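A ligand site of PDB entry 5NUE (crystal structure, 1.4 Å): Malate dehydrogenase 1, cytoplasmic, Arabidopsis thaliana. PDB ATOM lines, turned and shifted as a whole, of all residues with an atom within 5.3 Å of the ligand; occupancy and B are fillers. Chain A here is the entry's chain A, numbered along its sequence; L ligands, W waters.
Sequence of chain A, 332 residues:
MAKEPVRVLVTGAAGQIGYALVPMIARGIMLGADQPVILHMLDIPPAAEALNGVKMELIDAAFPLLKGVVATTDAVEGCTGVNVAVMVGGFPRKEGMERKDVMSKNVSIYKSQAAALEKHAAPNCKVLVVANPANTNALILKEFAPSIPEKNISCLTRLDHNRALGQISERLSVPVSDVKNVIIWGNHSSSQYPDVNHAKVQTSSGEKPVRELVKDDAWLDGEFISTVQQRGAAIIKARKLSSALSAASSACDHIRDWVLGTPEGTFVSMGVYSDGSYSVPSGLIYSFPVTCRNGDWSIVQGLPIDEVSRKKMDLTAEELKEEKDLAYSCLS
The backbone carbonyl oxygen (O) of Val 130 lies close to an oxygen (O14) of the ligand (3.1 Å). O14 of the ligand lies close to O of Leu 156, 3.5 Å away. C of Ala 14 touches O5 of the ligand, at 3.7 Å. Leu 42 touches the ligand. CG1 of Ile 44 touches O6 of the ligand (3.4 Å). Val 88 touches the ligand. Gly 89 touches the ligand (CA to O4, 3.3 Å). CZ of Phe 91 touches C6 of the ligand, 3.6 Å away. Pro 92 touches the ligand (CD to O1, 3.4 Å). CD1 of Ile 109 touches N2 of the ligand (3.7 Å). CA of Ala 131 touches O12 of the ligand (3.5 Å). Leu 159 touches the ligand (CB to N7, 3.8 Å). Ser 243 touches the ligand. Ala 247 touches the ligand (CB to C19, 3.7 Å). Hydrophobic or aromatic side chains within 4 Å of the ligand: Ile 17, Ile 44, Val 88, Phe 91, Pro 92, Ile 109, Val 130, Ala 131, Leu 156, Leu 159, His 188 and Ala 247. 23 residues have an atom within 4 Å of the ligand: Gly 12, Ala 14, Gly 15, Gln 16, Ile 17, Leu 42, Asp 43, Ile 44, Val 88, Gly 89, Gly 90, Phe 91, Pro 92, Ile 109, Gln 113, Val 130, Ala 131, Asn 132, Leu 156, Leu 159, His 188, Ser 243 and Ala 247.
An oxygen (O6) of the ligand lies within hydrogen-bond range of the side-chain carboxylate (OD1) of Asp 43 (2.6 Å). O8 of the ligand is in hydrogen-bond range of N of Ile 17 (2.8 Å). An oxygen (O2) of the ligand is in hydrogen-bond range of the backbone NH (N) of Gln 16, 2.9 Å away. NE2 of Gln 16 lies within hydrogen-bond range of O9 of the ligand (3.1 Å). O12 of the ligand is in hydrogen-bond range of N of Asn 132 (2.9 Å). An oxygen (O13) of the ligand sits at hydrogen-bond distance from the side-chain amide nitrogen (ND2) of Asn 132. N4 of the ligand lies within hydrogen-bond range of NE2 of Gln 113 (3.1 Å). A nitrogen (N7) of the ligand sits close to a ring nitrogen (NE2) of His 188 (3.3 Å). An oxygen (O4) of the ligand sits at hydrogen-bond distance from the backbone NH (N) of Gly 90, at 3.2 Å. N5 of the ligand lies within hydrogen-bond range of N of Gly 12 (3.4 Å). N of Gly 15 lies within hydrogen-bond range of O5 of the ligand, at 3.4 Å.
Water W2 lies within hydrogen-bond range of the side-chain hydroxyl of Ser 242 (2.5 Å), an oxygen (O9) of the ligand (2.6 Å) and the backbone carbonyl oxygen of Ser 243 (2.7 Å). Water W4 lies within hydrogen-bond range of O9 of the ligand (2.7 Å) and NE2 of Gln 16 (3.3 Å). Water W7 bridges O13 of the ligand (2.7 Å) and OG of Ser 242 (2.8 Å). Water W9 lies within hydrogen-bond range of O of Phe 91, O12 of the ligand, O of Asn 132 and ND2 of Asn 106. Water W3 lies within hydrogen-bond range of N7 of the ligand, O of Leu 156, N of Leu 159 and ND1 of His 188. Water W14 bridges O of Gly 90 and O1 of the ligand.
The side-chain carboxylate of Asp 43 lies within hydrogen-bond range of the backbone NH of Ala 13 (3.4 Å). The backbone carbonyl oxygen (O) of Ser 242 lies within hydrogen-bond range of the side-chain amide nitrogen (NE2) of Gln 16. The side-chain amide oxygen (OD1) of Asn 132 lies close to the backbone NH (N) of Ala 134. The side-chain hydroxyl (OG1) of Thr 11 is in hydrogen-bond range of the backbone NH (N) of Gly 89 (3.1 Å). O of Leu 42 sits at hydrogen-bond distance from N of Gly 12 (2.9 Å). The backbone carbonyl oxygen (O) of Val 129 lies within hydrogen-bond range of the backbone NH (N) of Leu 156 (3.0 Å). OD1 of Asn 106 is in hydrogen-bond range of N of Phe 91 (2.8 Å). N of Ala 13 is in hydrogen-bond range of O of Leu 42.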
ATOM      1  N   THR A  11      -2.316 -17.775 -23.075  1.00  0.00           N
ATOM      2  CA  THR A  11      -1.548 -16.779 -22.343  1.00  0.00           C
ATOM      3  C   THR A  11      -2.327 -15.465 -22.355  1.00  0.00           C
ATOM      4  O   THR A  11      -3.224 -15.270 -23.182  1.00  0.00           O
ATOM      5  CB  THR A  11      -0.136 -16.571 -22.896  1.00  0.00           C
ATOM      6  OG1 THR A  11      -0.268 -15.853 -24.140  1.00  0.00           O
ATOM      7  CG2 THR A  11       0.579 -17.875 -23.132  1.00  0.00           C
ATOM      8  N   GLY A  12      -1.992 -14.556 -21.434  1.00  0.00           N
ATOM      9  CA  GLY A  12      -2.838 -13.377 -21.234  1.00  0.00           C
ATOM     10  C   GLY A  12      -4.227 -13.720 -20.710  1.00  0.00           C
ATOM     11  O   GLY A  12      -5.183 -12.958 -20.930  1.00  0.00           O
ATOM     12  N   ALA A  13      -4.353 -14.827 -19.993  1.00  0.00           N
ATOM     13  CA  ALA A  13      -5.675 -15.379 -19.718  1.00  0.00           C
ATOM     14  C   ALA A  13      -6.506 -14.524 -18.753  1.00  0.00           C
ATOM     15  O   ALA A  13      -7.725 -14.700 -18.687  1.00  0.00           O
ATOM     16  CB  ALA A  13      -5.490 -16.814 -19.202  1.00  0.00           C
ATOM     17  N   ALA A  14      -5.882 -13.643 -17.974  1.00  0.00           N
ATOM     18  CA  ALA A  14      -6.613 -12.778 -17.047  1.00  0.00           C
ATOM     19  C   ALA A  14      -7.118 -11.485 -17.699  1.00  0.00           C
ATOM     20  O   ALA A  14      -7.736 -10.662 -17.008  1.00  0.00           O
ATOM     21  CB  ALA A  14      -5.759 -12.434 -15.808  1.00  0.00           C
ATOM     22  N   GLY A  15      -6.879 -11.283 -18.990  1.00  0.00           N
ATOM     23  CA  GLY A  15      -7.288 -10.069 -19.670  1.00  0.00           C
ATOM     24  C   GLY A  15      -8.622 -10.214 -20.383  1.00  0.00           C
ATOM     25  O   GLY A  15      -9.365 -11.193 -20.233  1.00  0.00           O
ATOM     26  N   GLN A  16      -8.920  -9.192 -21.180  1.00  0.00           N
ATOM     27  CA  GLN A  16     -10.228  -9.089 -21.814  1.00  0.00           C
ATOM     28  C   GLN A  16     -10.508 -10.235 -22.791  1.00  0.00           C
ATOM     29  O   GLN A  16     -11.560 -10.890 -22.746  1.00  0.00           O
ATOM     30  CB  GLN A  16     -10.323  -7.754 -22.519  1.00  0.00           C
ATOM     31  CG  GLN A  16     -11.771  -7.407 -22.836  1.00  0.00           C
ATOM     32  CD  GLN A  16     -11.990  -6.245 -23.875  1.00  0.00           C
ATOM     33  OE1 GLN A  16     -13.139  -5.815 -24.031  1.00  0.00           O
ATOM     34  NE2 GLN A  16     -10.909  -5.800 -24.591  1.00  0.00           N
ATOM     35  N   ILE A  17      -9.595 -10.451 -23.738  1.00  0.00           N
ATOM     36  CA  ILE A  17      -9.759 -11.549 -24.701  1.00  0.00           C
ATOM     37  C   ILE A  17      -9.709 -12.898 -23.989  1.00  0.00           C
ATOM     38  O   ILE A  17     -10.524 -13.787 -24.278  1.00  0.00           O
ATOM     39  CB  ILE A  17      -8.718 -11.460 -25.826  1.00  0.00           C
ATOM     40  CG1 ILE A  17      -9.040 -10.267 -26.763  1.00  0.00           C
ATOM     41  CG2 ILE A  17      -8.746 -12.741 -26.649  1.00  0.00           C
ATOM     42  CD1 ILE A  17      -7.952 -10.023 -27.832  1.00  0.00           C
ATOM     43  N   GLY A  18      -8.771 -13.073 -23.044  1.00  0.00           N
ATOM     44  CA  GLY A  18      -8.717 -14.350 -22.323  1.00  0.00           C
ATOM     45  C   GLY A  18     -10.064 -14.685 -21.675  1.00  0.00           C
ATOM     46  O   GLY A  18     -10.505 -15.844 -21.683  1.00  0.00           O
ATOM     47  N   LEU A  42      -2.018 -18.800 -18.474  1.00  0.00           N
ATOM     48  CA  LEU A  42      -0.797 -18.107 -18.038  1.00  0.00           C
ATOM     49  C   LEU A  42      -1.046 -16.602 -18.034  1.00  0.00           C
ATOM     50  O   LEU A  42      -1.547 -16.060 -19.031  1.00  0.00           O
ATOM     51  CB  LEU A  42       0.316 -18.369 -19.034  1.00  0.00           C
ATOM     52  CG  LEU A  42       1.669 -17.692 -18.704  1.00  0.00           C
ATOM     53  CD1 LEU A  42       2.305 -18.275 -17.410  1.00  0.00           C
ATOM     54  CD2 LEU A  42       2.637 -17.866 -19.865  1.00  0.00           C
ATOM     55  N   ASP A  43      -0.702 -15.941 -16.936  1.00  0.00           N
ATOM     56  CA  ASP A  43      -0.666 -14.471 -16.909  1.00  0.00           C
ATOM     57  C   ASP A  43       0.581 -14.063 -16.131  1.00  0.00           C
ATOM     58  O   ASP A  43       1.490 -14.878 -15.960  1.00  0.00           O
ATOM     59  CB  ASP A  43      -2.013 -13.875 -16.471  1.00  0.00           C
ATOM     60  CG  ASP A  43      -2.264 -12.491 -17.106  1.00  0.00           C
ATOM     61  OD1 ASP A  43      -1.510 -11.554 -16.807  1.00  0.00           O
ATOM     62  OD2 ASP A  43      -3.199 -12.356 -17.927  1.00  0.00           O
ATOM     63  N   ILE A  44       0.613 -12.828 -15.655  1.00  0.00           N
ATOM     64  CA  ILE A  44       1.789 -12.338 -14.933  1.00  0.00           C
ATOM     65  C   ILE A  44       1.385 -11.984 -13.510  1.00  0.00           C
ATOM     66  O   ILE A  44       0.184 -11.839 -13.209  1.00  0.00           O
ATOM     67  CB  ILE A  44       2.449 -11.133 -15.654  1.00  0.00           C
ATOM     68  CG1 ILE A  44       1.401 -10.083 -16.059  1.00  0.00           C
ATOM     69  CG2 ILE A  44       3.261 -11.606 -16.878  1.00  0.00           C
ATOM     70  CD1 ILE A  44       2.039  -8.743 -16.584  1.00  0.00           C
ATOM     71  N   ALA A  47      -1.500  -9.788 -12.185  1.00  0.00           N
ATOM     72  CA  ALA A  47      -2.849 -10.237 -12.487  1.00  0.00           C
ATOM     73  C   ALA A  47      -3.197 -11.563 -11.801  1.00  0.00           C
ATOM     74  O   ALA A  47      -4.230 -12.163 -12.136  1.00  0.00           O
ATOM     75  CB  ALA A  47      -3.003 -10.376 -13.999  1.00  0.00           C
ATOM     76  N   VAL A  88      -2.192 -14.660 -26.157  1.00  0.00           N
ATOM     77  CA  VAL A  88      -2.882 -13.377 -26.030  1.00  0.00           C
ATOM     78  C   VAL A  88      -2.136 -12.438 -25.085  1.00  0.00           C
ATOM     79  O   VAL A  88      -2.495 -11.266 -24.989  1.00  0.00           O
ATOM     80  CB  VAL A  88      -4.351 -13.618 -25.587  1.00  0.00           C
ATOM     81  CG1 VAL A  88      -5.172 -12.413 -25.765  1.00  0.00           C
ATOM     82  CG2 VAL A  88      -4.916 -14.866 -26.330  1.00  0.00           C
ATOM     83  N   GLY A  89      -1.114 -12.913 -24.404  1.00  0.00           N
ATOM     84  CA  GLY A  89      -0.420 -12.061 -23.461  1.00  0.00           C
ATOM     85  C   GLY A  89       0.247 -10.887 -24.165  1.00  0.00           C
ATOM     86  O   GLY A  89       0.865 -11.036 -25.224  1.00  0.00           O
ATOM     87  N   GLY A  90       0.134  -9.726 -23.565  1.00  0.00           N
ATOM     88  CA  GLY A  90       0.605  -8.524 -24.223  1.00  0.00           C
ATOM     89  C   GLY A  90       0.000  -7.290 -23.596  1.00  0.00           C
ATOM     90  O   GLY A  90      -0.635  -7.357 -22.542  1.00  0.00           O
ATOM     91  N   PHE A  91       0.314  -6.165 -24.229  1.00  0.00           N
ATOM     92  CA  PHE A  91      -0.089  -4.851 -23.737  1.00  0.00           C
ATOM     93  C   PHE A  91      -0.742  -4.139 -24.902  1.00  0.00           C
ATOM     94  O   PHE A  91      -0.025  -3.751 -25.857  1.00  0.00           O
ATOM     95  CB  PHE A  91       1.153  -4.135 -23.229  1.00  0.00           C
ATOM     96  CG  PHE A  91       1.733  -4.789 -22.029  1.00  0.00           C
ATOM     97  CD1 PHE A  91       1.176  -4.597 -20.780  1.00  0.00           C
ATOM     98  CD2 PHE A  91       2.807  -5.662 -22.157  1.00  0.00           C
ATOM     99  CE1 PHE A  91       1.715  -5.269 -19.640  1.00  0.00           C
ATOM    100  CE2 PHE A  91       3.371  -6.316 -21.048  1.00  0.00           C
ATOM    101  CZ  PHE A  91       2.812  -6.122 -19.777  1.00  0.00           C
ATOM    102  N   PRO A  92      -2.051  -3.898 -24.859  1.00  0.00           N
ATOM    103  CA  PRO A  92      -2.711  -3.192 -25.965  1.00  0.00           C
ATOM    104  C   PRO A  92      -2.290  -1.736 -25.980  1.00  0.00           C
ATOM    105  O   PRO A  92      -1.996  -1.126 -24.946  1.00  0.00           O
ATOM    106  CB  PRO A  92      -4.198  -3.343 -25.637  1.00  0.00           C
ATOM    107  CG  PRO A  92      -4.264  -3.630 -24.120  1.00  0.00           C
ATOM    108  CD  PRO A  92      -2.967  -4.369 -23.814  1.00  0.00           C
ATOM    109  N   ARG A  93      -2.288  -1.151 -27.164  1.00  0.00           N
ATOM    110  CA  ARG A  93      -1.851   0.227 -27.293  1.00  0.00           C
ATOM    111  C   ARG A  93      -2.852   1.126 -26.595  1.00  0.00           C
ATOM    112  O   ARG A  93      -4.078   0.939 -26.718  1.00  0.00           O
ATOM    113  CB  ARG A  93      -1.725   0.632 -28.770  1.00  0.00           C
ATOM    114  CG  ARG A  93      -1.219   2.082 -28.930  1.00  0.00           C
ATOM    115  N   ASN A 106       5.798  -5.620 -26.241  1.00  0.00           N
ATOM    116  CA  ASN A 106       5.170  -6.878 -26.656  1.00  0.00           C
ATOM    117  C   ASN A 106       6.151  -7.887 -27.248  1.00  0.00           C
ATOM    118  O   ASN A 106       6.100  -9.071 -26.866  1.00  0.00           O
ATOM    119  CB  ASN A 106       4.032  -6.556 -27.640  1.00  0.00           C
ATOM    120  CG  ASN A 106       2.832  -5.985 -26.942  1.00  0.00           C
ATOM    121  OD1 ASN A 106       2.113  -6.708 -26.256  1.00  0.00           O
ATOM    122  ND2 ASN A 106       2.642  -4.656 -27.052  1.00  0.00           N
ATOM    123  N   ILE A 109       8.029 -10.282 -24.910  1.00  0.00           N
ATOM    124  CA  ILE A 109       7.300 -11.447 -24.382  1.00  0.00           C
ATOM    125  C   ILE A 109       7.520 -12.645 -25.282  1.00  0.00           C
ATOM    126  O   ILE A 109       7.703 -13.784 -24.791  1.00  0.00           O
ATOM    127  CB  ILE A 109       5.791 -11.123 -24.328  1.00  0.00           C
ATOM    128  CG1 ILE A 109       5.500  -9.930 -23.400  1.00  0.00           C
ATOM    129  CG2 ILE A 109       4.978 -12.375 -23.947  1.00  0.00           C
ATOM    130  CD1 ILE A 109       4.051  -9.464 -23.505  1.00  0.00           C
ATOM    131  N   GLN A 113       9.021 -16.254 -24.355  1.00  0.00           N
ATOM    132  CA  GLN A 113       8.168 -17.440 -24.270  1.00  0.00           C
ATOM    133  C   GLN A 113       8.450 -18.461 -25.354  1.00  0.00           C
ATOM    134  O   GLN A 113       8.101 -19.627 -25.184  1.00  0.00           O
ATOM    135  CB  GLN A 113       6.713 -17.007 -24.269  1.00  0.00           C
ATOM    136  CG  GLN A 113       6.358 -16.284 -22.994  1.00  0.00           C
ATOM    137  CD  GLN A 113       4.926 -15.818 -22.971  1.00  0.00           C
ATOM    138  OE1 GLN A 113       4.230 -15.889 -23.971  1.00  0.00           O
ATOM    139  NE2 GLN A 113       4.477 -15.355 -21.815  1.00  0.00           N
ATOM    140  N   VAL A 129      -0.697 -16.767 -32.486  1.00  0.00           N
ATOM    141  CA  VAL A 129      -0.424 -15.517 -31.791  1.00  0.00           C
ATOM    142  C   VAL A 129      -1.558 -14.537 -32.080  1.00  0.00           C
ATOM    143  O   VAL A 129      -1.812 -14.195 -33.243  1.00  0.00           O
ATOM    144  CB  VAL A 129       0.930 -14.915 -32.224  1.00  0.00           C
ATOM    145  CG1 VAL A 129       1.169 -13.586 -31.484  1.00  0.00           C
ATOM    146  CG2 VAL A 129       2.053 -15.897 -31.846  1.00  0.00           C
ATOM    147  N   VAL A 130      -2.196 -14.052 -31.025  1.00  0.00           N
ATOM    148  CA  VAL A 130      -3.256 -13.052 -31.108  1.00  0.00           C
ATOM    149  C   VAL A 130      -2.733 -11.660 -30.750  1.00  0.00           C
ATOM    150  O   VAL A 130      -3.089 -10.692 -31.399  1.00  0.00           O
ATOM    151  CB  VAL A 130      -4.430 -13.459 -30.203  1.00  0.00           C
ATOM    152  CG1 VAL A 130      -5.543 -12.338 -30.159  1.00  0.00           C
ATOM    153  CG2 VAL A 130      -5.025 -14.845 -30.633  1.00  0.00           C
ATOM    154  N   ALA A 131      -1.889 -11.579 -29.718  1.00  0.00           N
ATOM    155  CA  ALA A 131      -1.448 -10.286 -29.207  1.00  0.00           C
ATOM    156  C   ALA A 131      -0.794  -9.453 -30.302  1.00  0.00           C
ATOM    157  O   ALA A 131      -0.032  -9.971 -31.153  1.00  0.00           O
ATOM    158  CB  ALA A 131      -0.445 -10.498 -28.061  1.00  0.00           C
ATOM    159  N   ASN A 132      -1.052  -8.094 -30.243  1.00  0.00           N
ATOM    160  CA  ASN A 132      -0.515  -7.256 -31.302  1.00  0.00           C
ATOM    161  C   ASN A 132       0.876  -6.725 -30.954  1.00  0.00           C
ATOM    162  O   ASN A 132       1.212  -6.595 -29.788  1.00  0.00           O
ATOM    163  CB  ASN A 132      -1.461  -6.067 -31.547  1.00  0.00           C
ATOM    164  CG  ASN A 132      -2.673  -6.478 -32.354  1.00  0.00           C
ATOM    165  OD1 ASN A 132      -2.559  -7.373 -33.180  1.00  0.00           O
ATOM    166  ND2 ASN A 132      -3.841  -5.874 -32.092  1.00  0.00           N
ATOM    167  N   ALA A 134       0.406  -8.643 -34.223  1.00  0.00           N
ATOM    168  CA  ALA A 134       0.254 -10.110 -34.273  1.00  0.00           C
ATOM    169  C   ALA A 134       1.303 -10.769 -35.187  1.00  0.00           C
ATOM    170  O   ALA A 134       1.978 -11.739 -34.784  1.00  0.00           O
ATOM    171  CB  ALA A 134      -1.183 -10.490 -34.658  1.00  0.00           C
ATOM    172  N   LEU A 156      -3.205 -14.331 -35.908  1.00  0.00           N
ATOM    173  CA  LEU A 156      -4.647 -14.167 -36.148  1.00  0.00           C
ATOM    174  C   LEU A 156      -4.924 -13.022 -37.113  1.00  0.00           C
ATOM    175  O   LEU A 156      -4.835 -11.846 -36.728  1.00  0.00           O
ATOM    176  CB  LEU A 156      -5.342 -13.889 -34.812  1.00  0.00           C
ATOM    177  CG  LEU A 156      -6.868 -13.989 -34.927  1.00  0.00           C
ATOM    178  CD1 LEU A 156      -7.316 -15.451 -35.147  1.00  0.00           C
ATOM    179  CD2 LEU A 156      -7.543 -13.407 -33.692  1.00  0.00           C
ATOM    180  N   LEU A 159      -9.959 -12.497 -37.541  1.00  0.00           N
ATOM    181  CA  LEU A 159     -10.923 -11.440 -37.221  1.00  0.00           C
ATOM    182  C   LEU A 159     -11.041 -10.464 -38.361  1.00  0.00           C
ATOM    183  O   LEU A 159     -12.139 -10.052 -38.710  1.00  0.00           O
ATOM    184  CB  LEU A 159     -10.571 -10.732 -35.901  1.00  0.00           C
ATOM    185  CG  LEU A 159     -11.488  -9.559 -35.545  1.00  0.00           C
ATOM    186  CD1 LEU A 159     -13.001  -9.987 -35.474  1.00  0.00           C
ATOM    187  CD2 LEU A 159     -11.060  -8.925 -34.206  1.00  0.00           C
ATOM    188  N   HIS A 188      -1.869  -7.909 -40.077  1.00  0.00           N
ATOM    189  CA  HIS A 188      -3.009  -7.525 -39.227  1.00  0.00           C
ATOM    190  C   HIS A 188      -2.828  -6.051 -38.834  1.00  0.00           C
ATOM    191  O   HIS A 188      -2.328  -5.695 -37.761  1.00  0.00           O
ATOM    192  CB  HIS A 188      -3.110  -8.428 -37.987  1.00  0.00           C
ATOM    193  CG  HIS A 188      -4.230  -8.045 -37.068  1.00  0.00           C
ATOM    194  ND1 HIS A 188      -5.553  -8.170 -37.440  1.00  0.00           N
ATOM    195  CD2 HIS A 188      -4.225  -7.483 -35.836  1.00  0.00           C
ATOM    196  CE1 HIS A 188      -6.317  -7.713 -36.460  1.00  0.00           C
ATOM    197  NE2 HIS A 188      -5.541  -7.284 -35.471  1.00  0.00           N
ATOM    198  N   SER A 242     -10.466  -2.306 -27.101  1.00  0.00           N
ATOM    199  CA  SER A 242     -10.395  -3.044 -28.356  1.00  0.00           C
ATOM    200  C   SER A 242     -11.224  -4.340 -28.297  1.00  0.00           C
ATOM    201  O   SER A 242     -11.707  -4.773 -27.246  1.00  0.00           O
ATOM    202  CB  SER A 242      -8.926  -3.264 -28.744  1.00  0.00           C
ATOM    203  OG  SER A 242      -8.151  -3.780 -27.670  1.00  0.00           O
ATOM    204  N   SER A 243     -11.333  -4.985 -29.464  1.00  0.00           N
ATOM    205  CA  SER A 243     -12.214  -6.139 -29.631  1.00  0.00           C
ATOM    206  C   SER A 243     -11.837  -7.286 -28.698  1.00  0.00           C
ATOM    207  O   SER A 243     -10.650  -7.514 -28.392  1.00  0.00           O
ATOM    208  CB  SER A 243     -12.144  -6.635 -31.078  1.00  0.00           C
ATOM    209  OG  SER A 243     -10.856  -7.105 -31.394  1.00  0.00           O
ATOM    210  N   ALA A 247     -12.603 -11.136 -31.248  1.00  0.00           N
ATOM    211  CA  ALA A 247     -11.259 -11.700 -31.333  1.00  0.00           C
ATOM    212  C   ALA A 247     -11.248 -13.136 -30.807  1.00  0.00           C
ATOM    213  O   ALA A 247     -10.657 -14.013 -31.442  1.00  0.00           O
ATOM    214  CB  ALA A 247     -10.285 -10.791 -30.549  1.00  0.00           C
HETATM  215  P1  LIG L   1      -5.603  -7.090 -21.885  1.00  0.00           P
HETATM  216  O1  LIG L   1      -4.626  -6.059 -21.397  1.00  0.00           O
HETATM  217  O2  LIG L   1      -6.995  -7.057 -21.253  1.00  0.00           O
HETATM  218  O3  LIG L   1      -5.031  -8.595 -21.730  1.00  0.00           O
HETATM  219  C1  LIG L   1      -3.675  -8.849 -21.900  1.00  0.00           C
HETATM  220  C2  LIG L   1      -3.256  -9.682 -20.694  1.00  0.00           C
HETATM  221  O4  LIG L   1      -1.821 -10.206 -21.094  1.00  0.00           O
HETATM  222  C3  LIG L   1      -3.148  -9.048 -19.500  1.00  0.00           C
HETATM  223  O5  LIG L   1      -3.899  -9.754 -18.421  1.00  0.00           O
HETATM  224  C4  LIG L   1      -1.639  -9.111 -19.114  1.00  0.00           C
HETATM  225  O6  LIG L   1      -1.357  -9.088 -17.741  1.00  0.00           O
HETATM  226  C5  LIG L   1      -1.183 -10.369 -19.934  1.00  0.00           C
HETATM  227  N1  LIG L   1       0.275 -10.269 -20.054  1.00  0.00           N
HETATM  228  C6  LIG L   1       1.205  -9.311 -20.175  1.00  0.00           C
HETATM  229  N2  LIG L   1       2.401  -9.910 -20.259  1.00  0.00           N
HETATM  230  C7  LIG L   1       2.210 -11.242 -20.205  1.00  0.00           C
HETATM  231  C8  LIG L   1       3.124 -12.254 -20.213  1.00  0.00           C
HETATM  232  N3  LIG L   1       4.567 -12.104 -20.302  1.00  0.00           N
HETATM  233  N4  LIG L   1       2.699 -13.502 -20.142  1.00  0.00           N
HETATM  234  C9  LIG L   1       1.356 -13.733 -20.031  1.00  0.00           C
HETATM  235  N5  LIG L   1       0.432 -12.750 -19.981  1.00  0.00           N
HETATM  236  C10 LIG L   1       0.876 -11.480 -20.075  1.00  0.00           C
HETATM  237  O7  LIG L   1      -5.711  -6.883 -23.490  1.00  0.00           O
HETATM  238  P2  LIG L   1      -6.771  -7.609 -24.474  1.00  0.00           P
HETATM  239  O8  LIG L   1      -7.170  -8.987 -23.983  1.00  0.00           O
HETATM  240  O9  LIG L   1      -7.875  -6.615 -24.789  1.00  0.00           O
HETATM  241  O10 LIG L   1      -5.856  -7.769 -25.798  1.00  0.00           O
HETATM  242  C11 LIG L   1      -4.834  -8.700 -25.750  1.00  0.00           C
HETATM  243  C12 LIG L   1      -3.939  -8.588 -27.027  1.00  0.00           C
HETATM  244  O11 LIG L   1      -4.633  -8.931 -28.164  1.00  0.00           O
HETATM  245  C13 LIG L   1      -3.415  -7.152 -27.244  1.00  0.00           C
HETATM  246  O12 LIG L   1      -2.109  -7.191 -27.702  1.00  0.00           O
HETATM  247  C14 LIG L   1      -4.394  -6.703 -28.356  1.00  0.00           C
HETATM  248  O13 LIG L   1      -3.850  -5.509 -29.057  1.00  0.00           O
HETATM  249  C15 LIG L   1      -4.481  -7.772 -29.198  1.00  0.00           C
HETATM  250  N6  LIG L   1      -5.633  -7.937 -30.099  1.00  0.00           N
HETATM  251  C16 LIG L   1      -5.430  -8.677 -31.240  1.00  0.00           C
HETATM  252  C17 LIG L   1      -6.489  -8.904 -32.093  1.00  0.00           C
HETATM  253  C18 LIG L   1      -6.194  -9.681 -33.365  1.00  0.00           C
HETATM  254  O14 LIG L   1      -5.101 -10.200 -33.674  1.00  0.00           O
HETATM  255  N7  LIG L   1      -7.251  -9.768 -34.214  1.00  0.00           N
HETATM  256  C19 LIG L   1      -7.708  -8.361 -31.773  1.00  0.00           C
HETATM  257  C20 LIG L   1      -7.936  -7.626 -30.642  1.00  0.00           C
HETATM  258  C21 LIG L   1      -6.851  -7.419 -29.767  1.00  0.00           C
HETATM  259  O   HOH W   1      -8.717  -4.580 -21.333  1.00  0.00           O
HETATM  260  O   HOH W   2      -8.528  -6.240 -27.310  1.00  0.00           O
HETATM  261  O   HOH W   3      -7.517 -10.931 -36.718  1.00  0.00           O
HETATM  262  O   HOH W   4      -8.143  -4.074 -23.993  1.00  0.00           O
HETATM  263  O   HOH W   5      -7.280  -6.566 -18.630  1.00  0.00           O
HETATM  264  O   HOH W   6       5.017  -9.089 -19.689  1.00  0.00           O
HETATM  265  O   HOH W   7      -5.604  -3.474 -28.690  1.00  0.00           O
HETATM  266  O   HOH W   8      -5.181  -3.569 -20.519  1.00  0.00           O
HETATM  267  O   HOH W   9      -0.539  -4.983 -28.252  1.00  0.00           O
HETATM  268  O   HOH W  10      -5.210  -7.981 -16.842  1.00  0.00           O
HETATM  269  O   HOH W  11       6.002 -14.944 -19.493  1.00  0.00           O
HETATM  270  O   HOH W  12      -6.643 -11.364 -22.645  1.00  0.00           O
HETATM  271  O   HOH W  13      -1.094  -7.036 -15.990  1.00  0.00           O
HETATM  272  O   HOH W  14      -1.946  -5.862 -20.637  1.00  0.00           O
